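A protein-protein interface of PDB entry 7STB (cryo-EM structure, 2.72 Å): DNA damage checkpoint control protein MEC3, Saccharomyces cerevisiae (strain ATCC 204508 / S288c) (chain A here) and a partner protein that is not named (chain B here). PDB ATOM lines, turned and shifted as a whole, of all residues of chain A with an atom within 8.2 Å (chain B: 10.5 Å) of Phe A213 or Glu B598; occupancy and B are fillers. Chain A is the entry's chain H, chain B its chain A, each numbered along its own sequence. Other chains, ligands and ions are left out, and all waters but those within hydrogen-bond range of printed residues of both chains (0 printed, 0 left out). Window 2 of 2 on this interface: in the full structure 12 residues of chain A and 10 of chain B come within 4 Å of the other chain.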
ATOM      1  N   ARG A  36      18.824  35.551   5.712  1.00  0.00           N
ATOM      2  CA  ARG A  36      17.471  35.083   5.994  1.00  0.00           C
ATOM      3  C   ARG A  36      16.656  35.212   4.715  1.00  0.00           C
ATOM      4  O   ARG A  36      16.371  36.327   4.265  1.00  0.00           O
ATOM      5  CB  ARG A  36      16.829  35.887   7.122  1.00  0.00           C
ATOM      6  CG  ARG A  36      17.345  35.575   8.513  1.00  0.00           C
ATOM      7  CD  ARG A  36      16.531  36.324   9.556  1.00  0.00           C
ATOM      8  NE  ARG A  36      17.176  36.348  10.862  1.00  0.00           N
ATOM      9  CZ  ARG A  36      16.797  37.123  11.870  1.00  0.00           C
ATOM     10  NH1 ARG A  36      15.775  37.954  11.758  1.00  0.00           N
ATOM     11  NH2 ARG A  36      17.462  37.061  13.020  1.00  0.00           N
ATOM     12  N   SER A  51      26.718  32.680  15.128  1.00  0.00           N
ATOM     13  CA  SER A  51      26.654  31.295  15.581  1.00  0.00           C
ATOM     14  C   SER A  51      28.028  30.639  15.509  1.00  0.00           C
ATOM     15  O   SER A  51      28.772  30.839  14.548  1.00  0.00           O
ATOM     16  CB  SER A  51      25.648  30.503  14.744  1.00  0.00           C
ATOM     17  OG  SER A  51      25.855  30.715  13.358  1.00  0.00           O
ATOM     18  N   ARG A  86       9.442  25.863   8.289  1.00  0.00           N
ATOM     19  CA  ARG A  86       9.296  26.849   9.348  1.00  0.00           C
ATOM     20  C   ARG A  86       8.239  27.884   8.970  1.00  0.00           C
ATOM     21  O   ARG A  86       7.768  27.948   7.832  1.00  0.00           O
ATOM     22  CB  ARG A  86      10.634  27.534   9.630  1.00  0.00           C
ATOM     23  CG  ARG A  86      11.598  26.693  10.449  1.00  0.00           C
ATOM     24  CD  ARG A  86      12.977  27.333  10.513  1.00  0.00           C
ATOM     25  NE  ARG A  86      12.919  28.711  10.986  1.00  0.00           N
ATOM     26  CZ  ARG A  86      13.973  29.507  11.110  1.00  0.00           C
ATOM     27  NH1 ARG A  86      15.192  29.094  10.801  1.00  0.00           N
ATOM     28  NH2 ARG A  86      13.801  30.748  11.556  1.00  0.00           N
ATOM     29  N   ILE A  91      14.321  30.626   5.867  1.00  0.00           N
ATOM     30  CA  ILE A  91      15.534  29.814   5.842  1.00  0.00           C
ATOM     31  C   ILE A  91      16.692  30.703   6.272  1.00  0.00           C
ATOM     32  O   ILE A  91      16.968  31.721   5.627  1.00  0.00           O
ATOM     33  CB  ILE A  91      15.790  29.212   4.451  1.00  0.00           C
ATOM     34  CG1 ILE A  91      14.655  28.261   4.067  1.00  0.00           C
ATOM     35  CG2 ILE A  91      17.126  28.474   4.426  1.00  0.00           C
ATOM     36  CD1 ILE A  91      14.683  27.821   2.617  1.00  0.00           C
ATOM     37  N   THR A  92      17.372  30.319   7.347  1.00  0.00           N
ATOM     38  CA  THR A  92      18.473  31.097   7.898  1.00  0.00           C
ATOM     39  C   THR A  92      19.788  30.382   7.628  1.00  0.00           C
ATOM     40  O   THR A  92      19.904  29.174   7.862  1.00  0.00           O
ATOM     41  CB  THR A  92      18.294  31.319   9.401  1.00  0.00           C
ATOM     42  OG1 THR A  92      16.942  31.707   9.671  1.00  0.00           O
ATOM     43  CG2 THR A  92      19.240  32.403   9.891  1.00  0.00           C
ATOM     44  N   MET A  93      20.774  31.131   7.137  1.00  0.00           N
ATOM     45  CA  MET A  93      22.061  30.573   6.753  1.00  0.00           C
ATOM     46  C   MET A  93      23.178  31.480   7.247  1.00  0.00           C
ATOM     47  O   MET A  93      22.992  32.688   7.409  1.00  0.00           O
ATOM     48  CB  MET A  93      22.159  30.410   5.230  1.00  0.00           C
ATOM     49  CG  MET A  93      21.069  29.542   4.621  1.00  0.00           C
ATOM     50  SD  MET A  93      20.806  29.875   2.869  1.00  0.00           S
ATOM     51  CE  MET A  93      22.315  29.222   2.165  1.00  0.00           C
ATOM     52  N   ASN A 151      23.851  21.331  13.491  1.00  0.00           N
ATOM     53  CA  ASN A 151      24.234  22.385  12.559  1.00  0.00           C
ATOM     54  C   ASN A 151      24.690  21.796  11.228  1.00  0.00           C
ATOM     55  O   ASN A 151      25.887  21.739  10.949  1.00  0.00           O
ATOM     56  CB  ASN A 151      25.345  23.250  13.158  1.00  0.00           C
ATOM     57  CG  ASN A 151      24.876  24.055  14.354  1.00  0.00           C
ATOM     58  OD1 ASN A 151      25.337  23.846  15.476  1.00  0.00           O
ATOM     59  ND2 ASN A 151      23.955  24.982  14.119  1.00  0.00           N
ATOM     60  N   PRO A 152      23.736  21.357  10.408  1.00  0.00           N
ATOM     61  CA  PRO A 152      24.097  20.805   9.097  1.00  0.00           C
ATOM     62  C   PRO A 152      24.838  21.828   8.250  1.00  0.00           C
ATOM     63  O   PRO A 152      24.558  23.026   8.303  1.00  0.00           O
ATOM     64  CB  PRO A 152      22.743  20.433   8.480  1.00  0.00           C
ATOM     65  CG  PRO A 152      21.805  20.317   9.633  1.00  0.00           C
ATOM     66  CD  PRO A 152      22.288  21.292  10.660  1.00  0.00           C
ATOM     67  N   LYS A 210      26.348  27.315   6.480  1.00  0.00           N
ATOM     68  CA  LYS A 210      25.868  26.586   7.648  1.00  0.00           C
ATOM     69  C   LYS A 210      24.401  26.913   7.887  1.00  0.00           C
ATOM     70  O   LYS A 210      24.040  28.085   8.023  1.00  0.00           O
ATOM     71  CB  LYS A 210      26.697  26.938   8.886  1.00  0.00           C
ATOM     72  CG  LYS A 210      26.548  25.958  10.036  1.00  0.00           C
ATOM     73  CD  LYS A 210      26.674  26.652  11.384  1.00  0.00           C
ATOM     74  CE  LYS A 210      28.038  27.307  11.559  1.00  0.00           C
ATOM     75  NZ  LYS A 210      28.136  28.051  12.844  1.00  0.00           N
ATOM     76  N   LEU A 211      23.562  25.882   7.943  1.00  0.00           N
ATOM     77  CA  LEU A 211      22.155  26.090   8.256  1.00  0.00           C
ATOM     78  C   LEU A 211      22.000  26.402   9.738  1.00  0.00           C
ATOM     79  O   LEU A 211      22.546  25.697  10.592  1.00  0.00           O
ATOM     80  CB  LEU A 211      21.337  24.857   7.881  1.00  0.00           C
ATOM     81  CG  LEU A 211      20.762  24.863   6.463  1.00  0.00           C
ATOM     82  CD1 LEU A 211      21.880  24.877   5.434  1.00  0.00           C
ATOM     83  CD2 LEU A 211      19.849  23.667   6.250  1.00  0.00           C
ATOM     84  N   LEU A 212      21.252  27.457  10.044  1.00  0.00           N
ATOM     85  CA  LEU A 212      21.131  27.955  11.406  1.00  0.00           C
ATOM     86  C   LEU A 212      19.791  27.528  11.992  1.00  0.00           C
ATOM     87  O   LEU A 212      18.770  27.522  11.297  1.00  0.00           O
ATOM     88  CB  LEU A 212      21.260  29.480  11.437  1.00  0.00           C
ATOM     89  CG  LEU A 212      21.224  30.133  12.820  1.00  0.00           C
ATOM     90  CD1 LEU A 212      22.409  29.649  13.636  1.00  0.00           C
ATOM     91  CD2 LEU A 212      21.230  31.648  12.718  1.00  0.00           C
ATOM     92  N   PHE A 213      19.800  27.169  13.273  1.00  0.00           N
ATOM     93  CA  PHE A 213      18.595  26.680  13.924  1.00  0.00           C
ATOM     94  C   PHE A 213      17.573  27.802  14.089  1.00  0.00           C
ATOM     95  O   PHE A 213      17.901  28.992  14.073  1.00  0.00           O
ATOM     96  CB  PHE A 213      18.930  26.075  15.288  1.00  0.00           C
ATOM     97  CG  PHE A 213      19.479  24.680  15.212  1.00  0.00           C
ATOM     98  CD1 PHE A 213      18.642  23.606  14.963  1.00  0.00           C
ATOM     99  CD2 PHE A 213      20.831  24.442  15.392  1.00  0.00           C
ATOM    100  CE1 PHE A 213      19.143  22.320  14.893  1.00  0.00           C
ATOM    101  CE2 PHE A 213      21.338  23.159  15.323  1.00  0.00           C
ATOM    102  CZ  PHE A 213      20.493  22.096  15.073  1.00  0.00           C
ATOM    103  N   ARG A 214      16.309  27.401  14.252  1.00  0.00           N
ATOM    104  CA  ARG A 214      15.230  28.375  14.376  1.00  0.00           C
ATOM    105  C   ARG A 214      15.423  29.260  15.600  1.00  0.00           C
ATOM    106  O   ARG A 214      15.284  30.486  15.523  1.00  0.00           O
ATOM    107  CB  ARG A 214      13.884  27.652  14.443  1.00  0.00           C
ATOM    108  CG  ARG A 214      12.678  28.578  14.425  1.00  0.00           C
ATOM    109  CD  ARG A 214      11.376  27.794  14.468  1.00  0.00           C
ATOM    110  NE  ARG A 214      10.230  28.647  14.763  1.00  0.00           N
ATOM    111  CZ  ARG A 214       9.845  28.995  15.984  1.00  0.00           C
ATOM    112  NH1 ARG A 214      10.496  28.583  17.060  1.00  0.00           N
ATOM    113  NH2 ARG A 214       8.778  29.775  16.129  1.00  0.00           N
ATOM    114  N   ALA A 215      15.743  28.656  16.747  1.00  0.00           N
ATOM    115  CA  ALA A 215      15.947  29.443  17.959  1.00  0.00           C
ATOM    116  C   ALA A 215      17.148  30.368  17.818  1.00  0.00           C
ATOM    117  O   ALA A 215      17.094  31.540  18.215  1.00  0.00           O
ATOM    118  CB  ALA A 215      16.124  28.516  19.162  1.00  0.00           C
ATOM    119  N   GLN A 216      18.244  29.862  17.247  1.00  0.00           N
ATOM    120  CA  GLN A 216      19.428  30.693  17.062  1.00  0.00           C
ATOM    121  C   GLN A 216      19.134  31.865  16.135  1.00  0.00           C
ATOM    122  O   GLN A 216      19.598  32.986  16.374  1.00  0.00           O
ATOM    123  CB  GLN A 216      20.579  29.844  16.523  1.00  0.00           C
ATOM    124  CG  GLN A 216      21.086  28.809  17.518  1.00  0.00           C
ATOM    125  CD  GLN A 216      22.037  27.804  16.898  1.00  0.00           C
ATOM    126  OE1 GLN A 216      21.916  27.458  15.724  1.00  0.00           O
ATOM    127  NE2 GLN A 216      22.991  27.329  17.689  1.00  0.00           N
ATOM    128  N   ASP A 217      18.363  31.628  15.072  1.00  0.00           N
ATOM    129  CA  ASP A 217      17.938  32.729  14.214  1.00  0.00           C
ATOM    130  C   ASP A 217      17.082  33.724  14.985  1.00  0.00           C
ATOM    131  O   ASP A 217      17.233  34.941  14.827  1.00  0.00           O
ATOM    132  CB  ASP A 217      17.172  32.187  13.009  1.00  0.00           C
ATOM    133  CG  ASP A 217      16.689  33.285  12.085  1.00  0.00           C
ATOM    134  OD1 ASP A 217      17.428  34.273  11.897  1.00  0.00           O
ATOM    135  OD2 ASP A 217      15.570  33.161  11.545  1.00  0.00           O
ATOM    136  N   THR A 218      16.173  33.224  15.827  1.00  0.00           N
ATOM    137  CA  THR A 218      15.323  34.112  16.611  1.00  0.00           C
ATOM    138  C   THR A 218      16.137  34.952  17.586  1.00  0.00           C
ATOM    139  O   THR A 218      15.716  36.054  17.955  1.00  0.00           O
ATOM    140  CB  THR A 218      14.273  33.299  17.371  1.00  0.00           C
ATOM    141  OG1 THR A 218      13.547  32.472  16.451  1.00  0.00           O
ATOM    142  CG2 THR A 218      13.301  34.218  18.097  1.00  0.00           C
ATOM    143  N   ARG A 219      17.299  34.454  18.016  1.00  0.00           N
ATOM    144  CA  ARG A 219      18.113  35.211  18.963  1.00  0.00           C
ATOM    145  C   ARG A 219      18.543  36.551  18.377  1.00  0.00           C
ATOM    146  O   ARG A 219      18.509  37.577  19.067  1.00  0.00           O
ATOM    147  CB  ARG A 219      19.336  34.394  19.379  1.00  0.00           C
ATOM    148  CG  ARG A 219      19.013  33.223  20.290  1.00  0.00           C
ATOM    149  CD  ARG A 219      20.177  32.253  20.391  1.00  0.00           C
ATOM    150  NE  ARG A 219      19.727  30.881  20.596  1.00  0.00           N
ATOM    151  CZ  ARG A 219      20.536  29.837  20.723  1.00  0.00           C
ATOM    152  NH1 ARG A 219      21.851  29.973  20.679  1.00  0.00           N
ATOM    153  NH2 ARG A 219      20.010  28.628  20.898  1.00  0.00           N
ATOM    154  N   ARG B 575      24.642  25.274  27.259  1.00  0.00           N
ATOM    155  CA  ARG B 575      23.330  24.714  26.950  1.00  0.00           C
ATOM    156  C   ARG B 575      22.322  25.050  28.042  1.00  0.00           C
ATOM    157  O   ARG B 575      21.181  25.436  27.752  1.00  0.00           O
ATOM    158  CB  ARG B 575      23.441  23.200  26.767  1.00  0.00           C
ATOM    159  CG  ARG B 575      22.125  22.505  26.452  1.00  0.00           C
ATOM    160  CD  ARG B 575      22.313  21.002  26.329  1.00  0.00           C
ATOM    161  NE  ARG B 575      21.055  20.307  26.085  1.00  0.00           N
ATOM    162  CZ  ARG B 575      20.952  19.008  25.834  1.00  0.00           C
ATOM    163  NH1 ARG B 575      22.017  18.226  25.788  1.00  0.00           N
ATOM    164  NH2 ARG B 575      19.749  18.482  25.626  1.00  0.00           N
ATOM    165  N   ARG B 578      21.348  28.708  27.770  1.00  0.00           N
ATOM    166  CA  ARG B 578      20.405  28.938  26.680  1.00  0.00           C
ATOM    167  C   ARG B 578      19.007  28.466  27.057  1.00  0.00           C
ATOM    168  O   ARG B 578      18.015  29.157  26.788  1.00  0.00           O
ATOM    169  CB  ARG B 578      20.887  28.231  25.412  1.00  0.00           C
ATOM    170  CG  ARG B 578      22.154  28.825  24.817  1.00  0.00           C
ATOM    171  CD  ARG B 578      22.426  28.276  23.426  1.00  0.00           C
ATOM    172  NE  ARG B 578      22.411  26.818  23.393  1.00  0.00           N
ATOM    173  CZ  ARG B 578      23.475  26.046  23.572  1.00  0.00           C
ATOM    174  NH1 ARG B 578      24.671  26.560  23.816  1.00  0.00           N
ATOM    175  NH2 ARG B 578      23.337  24.726  23.510  1.00  0.00           N
ATOM    176  N   ASP B 582      15.693  30.830  27.381  1.00  0.00           N
ATOM    177  CA  ASP B 582      14.460  30.535  26.657  1.00  0.00           C
ATOM    178  C   ASP B 582      13.274  30.439  27.609  1.00  0.00           C
ATOM    179  O   ASP B 582      12.200  30.984  27.330  1.00  0.00           O
ATOM    180  CB  ASP B 582      14.617  29.237  25.864  1.00  0.00           C
ATOM    181  CG  ASP B 582      15.609  29.366  24.725  1.00  0.00           C
ATOM    182  OD1 ASP B 582      16.062  30.498  24.455  1.00  0.00           O
ATOM    183  OD2 ASP B 582      15.936  28.335  24.100  1.00  0.00           O
ATOM    184  N   GLU B 598      18.072  20.464  17.207  1.00  0.00           N
ATOM    185  CA  GLU B 598      16.884  19.933  16.550  1.00  0.00           C
ATOM    186  C   GLU B 598      17.227  19.382  15.169  1.00  0.00           C
ATOM    187  O   GLU B 598      16.534  19.659  14.190  1.00  0.00           O
ATOM    188  CB  GLU B 598      15.809  21.014  16.431  1.00  0.00           C
ATOM    189  N   GLU B 599      18.306  18.598  15.099  1.00  0.00           N
ATOM    190  CA  GLU B 599      18.697  17.998  13.828  1.00  0.00           C
ATOM    191  C   GLU B 599      17.626  17.049  13.306  1.00  0.00           C
ATOM    192  O   GLU B 599      17.552  16.801  12.096  1.00  0.00           O
ATOM    193  CB  GLU B 599      20.028  17.261  13.983  1.00  0.00           C
ATOM    194  N   THR B 600      16.794  16.509  14.198  1.00  0.00           N
ATOM    195  CA  THR B 600      15.710  15.637  13.761  1.00  0.00           C
ATOM    196  C   THR B 600      14.733  16.376  12.858  1.00  0.00           C
ATOM    197  O   THR B 600      14.231  15.802  11.885  1.00  0.00           O
ATOM    198  CB  THR B 600      14.975  15.060  14.971  1.00  0.00           C
ATOM    199  N   SER B 601      14.447  17.645  13.162  1.00  0.00           N
ATOM    200  CA  SER B 601      13.560  18.423  12.304  1.00  0.00           C
ATOM    201  C   SER B 601      14.140  18.564  10.903  1.00  0.00           C
ATOM    202  O   SER B 601      13.423  18.405   9.909  1.00  0.00           O
ATOM    203  CB  SER B 601      13.309  19.799  12.922  1.00  0.00           C
ATOM    204  OG  SER B 601      12.361  20.531  12.165  1.00  0.00           O
ATOM    205  N   PHE B 602      15.437  18.863  10.804  1.00  0.00           N
ATOM    206  CA  PHE B 602      16.072  18.964   9.494  1.00  0.00           C
ATOM    207  C   PHE B 602      16.037  17.629   8.764  1.00  0.00           C
ATOM    208  O   PHE B 602      15.763  17.578   7.558  1.00  0.00           O
ATOM    209  CB  PHE B 602      17.512  19.452   9.645  1.00  0.00           C
ATOM    210  CG  PHE B 602      18.268  19.518   8.348  1.00  0.00           C
ATOM    211  CD1 PHE B 602      17.964  20.483   7.402  1.00  0.00           C
ATOM    212  CD2 PHE B 602      19.280  18.614   8.074  1.00  0.00           C
ATOM    213  CE1 PHE B 602      18.657  20.546   6.208  1.00  0.00           C
ATOM    214  CE2 PHE B 602      19.976  18.672   6.880  1.00  0.00           C
ATOM    215  CZ  PHE B 602      19.664  19.638   5.948  1.00  0.00           C
ATOM    216  N   ASN B 603      16.314  16.535   9.476  1.00  0.00           N
ATOM    217  CA  ASN B 603      16.284  15.219   8.846  1.00  0.00           C
ATOM    218  C   ASN B 603      14.886  14.868   8.355  1.00  0.00           C
ATOM    219  O   ASN B 603      14.741  14.180   7.338  1.00  0.00           O
ATOM    220  CB  ASN B 603      16.782  14.158   9.827  1.00  0.00           C
ATOM    221  CG  ASN B 603      16.988  12.807   9.168  1.00  0.00           C
ATOM    222  OD1 ASN B 603      17.189  12.719   7.957  1.00  0.00           O
ATOM    223  ND2 ASN B 603      16.937  11.746   9.965  1.00  0.00           N
ATOM    224  N   ASP B 604      13.849  15.325   9.060  1.00  0.00           N
ATOM    225  CA  ASP B 604      12.481  15.017   8.664  1.00  0.00           C
ATOM    226  C   ASP B 604      12.092  15.684   7.353  1.00  0.00           C
ATOM    227  O   ASP B 604      11.156  15.220   6.693  1.00  0.00           O
ATOM    228  CB  ASP B 604      11.509  15.442   9.766  1.00  0.00           C
ATOM    229  CG  ASP B 604      11.621  14.581  11.008  1.00  0.00           C
ATOM    230  OD1 ASP B 604      12.274  13.518  10.941  1.00  0.00           O
ATOM    231  OD2 ASP B 604      11.056  14.966  12.053  1.00  0.00           O
ATOM    232  N   ASP B 605      12.781  16.754   6.961  1.00  0.00           N
ATOM    233  CA  ASP B 605      12.495  17.477   5.723  1.00  0.00           C
ATOM    234  C   ASP B 605      13.790  17.676   4.947  1.00  0.00           C
ATOM    235  O   ASP B 605      14.348  18.780   4.910  1.00  0.00           O
ATOM    236  CB  ASP B 605      11.817  18.817   6.015  1.00  0.00           C
ATOM    237  CG  ASP B 605      12.615  19.679   6.973  1.00  0.00           C
ATOM    238  OD1 ASP B 605      13.673  19.217   7.450  1.00  0.00           O
ATOM    239  OD2 ASP B 605      12.187  20.819   7.246  1.00  0.00           O
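Among the printed residues, 5 pairs touch across the chains.
Among the printed residues, no Asp or Glu carboxylate lies within 4 Å of a Lys or Arg side-chain nitrogen of the other chain.
Among the printed residues, pairs that only touch across the chains: Pro A152 with Phe B602 (3.4 Å), Leu A211 with Phe B602 (3.3 Å), Phe A213 with Glu B598 (3.2 Å), Phe A213 with Glu B599 (3.8 Å) and Arg A219 with Arg B578 (3.3 Å).
Arg A86 touches none of the printed residues of chain B.
Of the printed residues of chain B, Pro A152 touches Phe B602.
Of the printed residues of chain B, Leu A211 touches Phe B602 (3.3 Å).
No residue of chain B comes within 4 Å of Leu A212.
No residue of chain B comes within 4 Å of Asp A217.
Of the printed residues of chain B, Arg A219 touches Arg B578 (3.3 Å).
Printed residues of chain A within 4 Å of Arg B578: Arg A219 (3.3 Å).
Of chain A, only Phe A213 comes within 4 Å of Glu B598.
Glu B599 touches just one residue of chain A: Phe A213.
Of the printed residues of chain A, Phe B602 touches Pro A152 (3.4 Å) and Leu A211 (3.3 Å).
The nearest residue of chain B that does not touch Phe A213 is Phe B602 (6.2 Å).
The nearest printed residue of chain B that does not touch Arg A219 is Asp B582 (5.2 Å).
The backbone carbonyl oxygen (O) of Pro A152 lies within hydrogen-bond range of the backbone NH (N) of Leu A211 (3.0 Å).
N of Phe A213 lies close to OE1 of Gln A216 (3.3 Å).
O of Phe B602 sits close to OD1 of Asp B605, 2.7 Å away.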
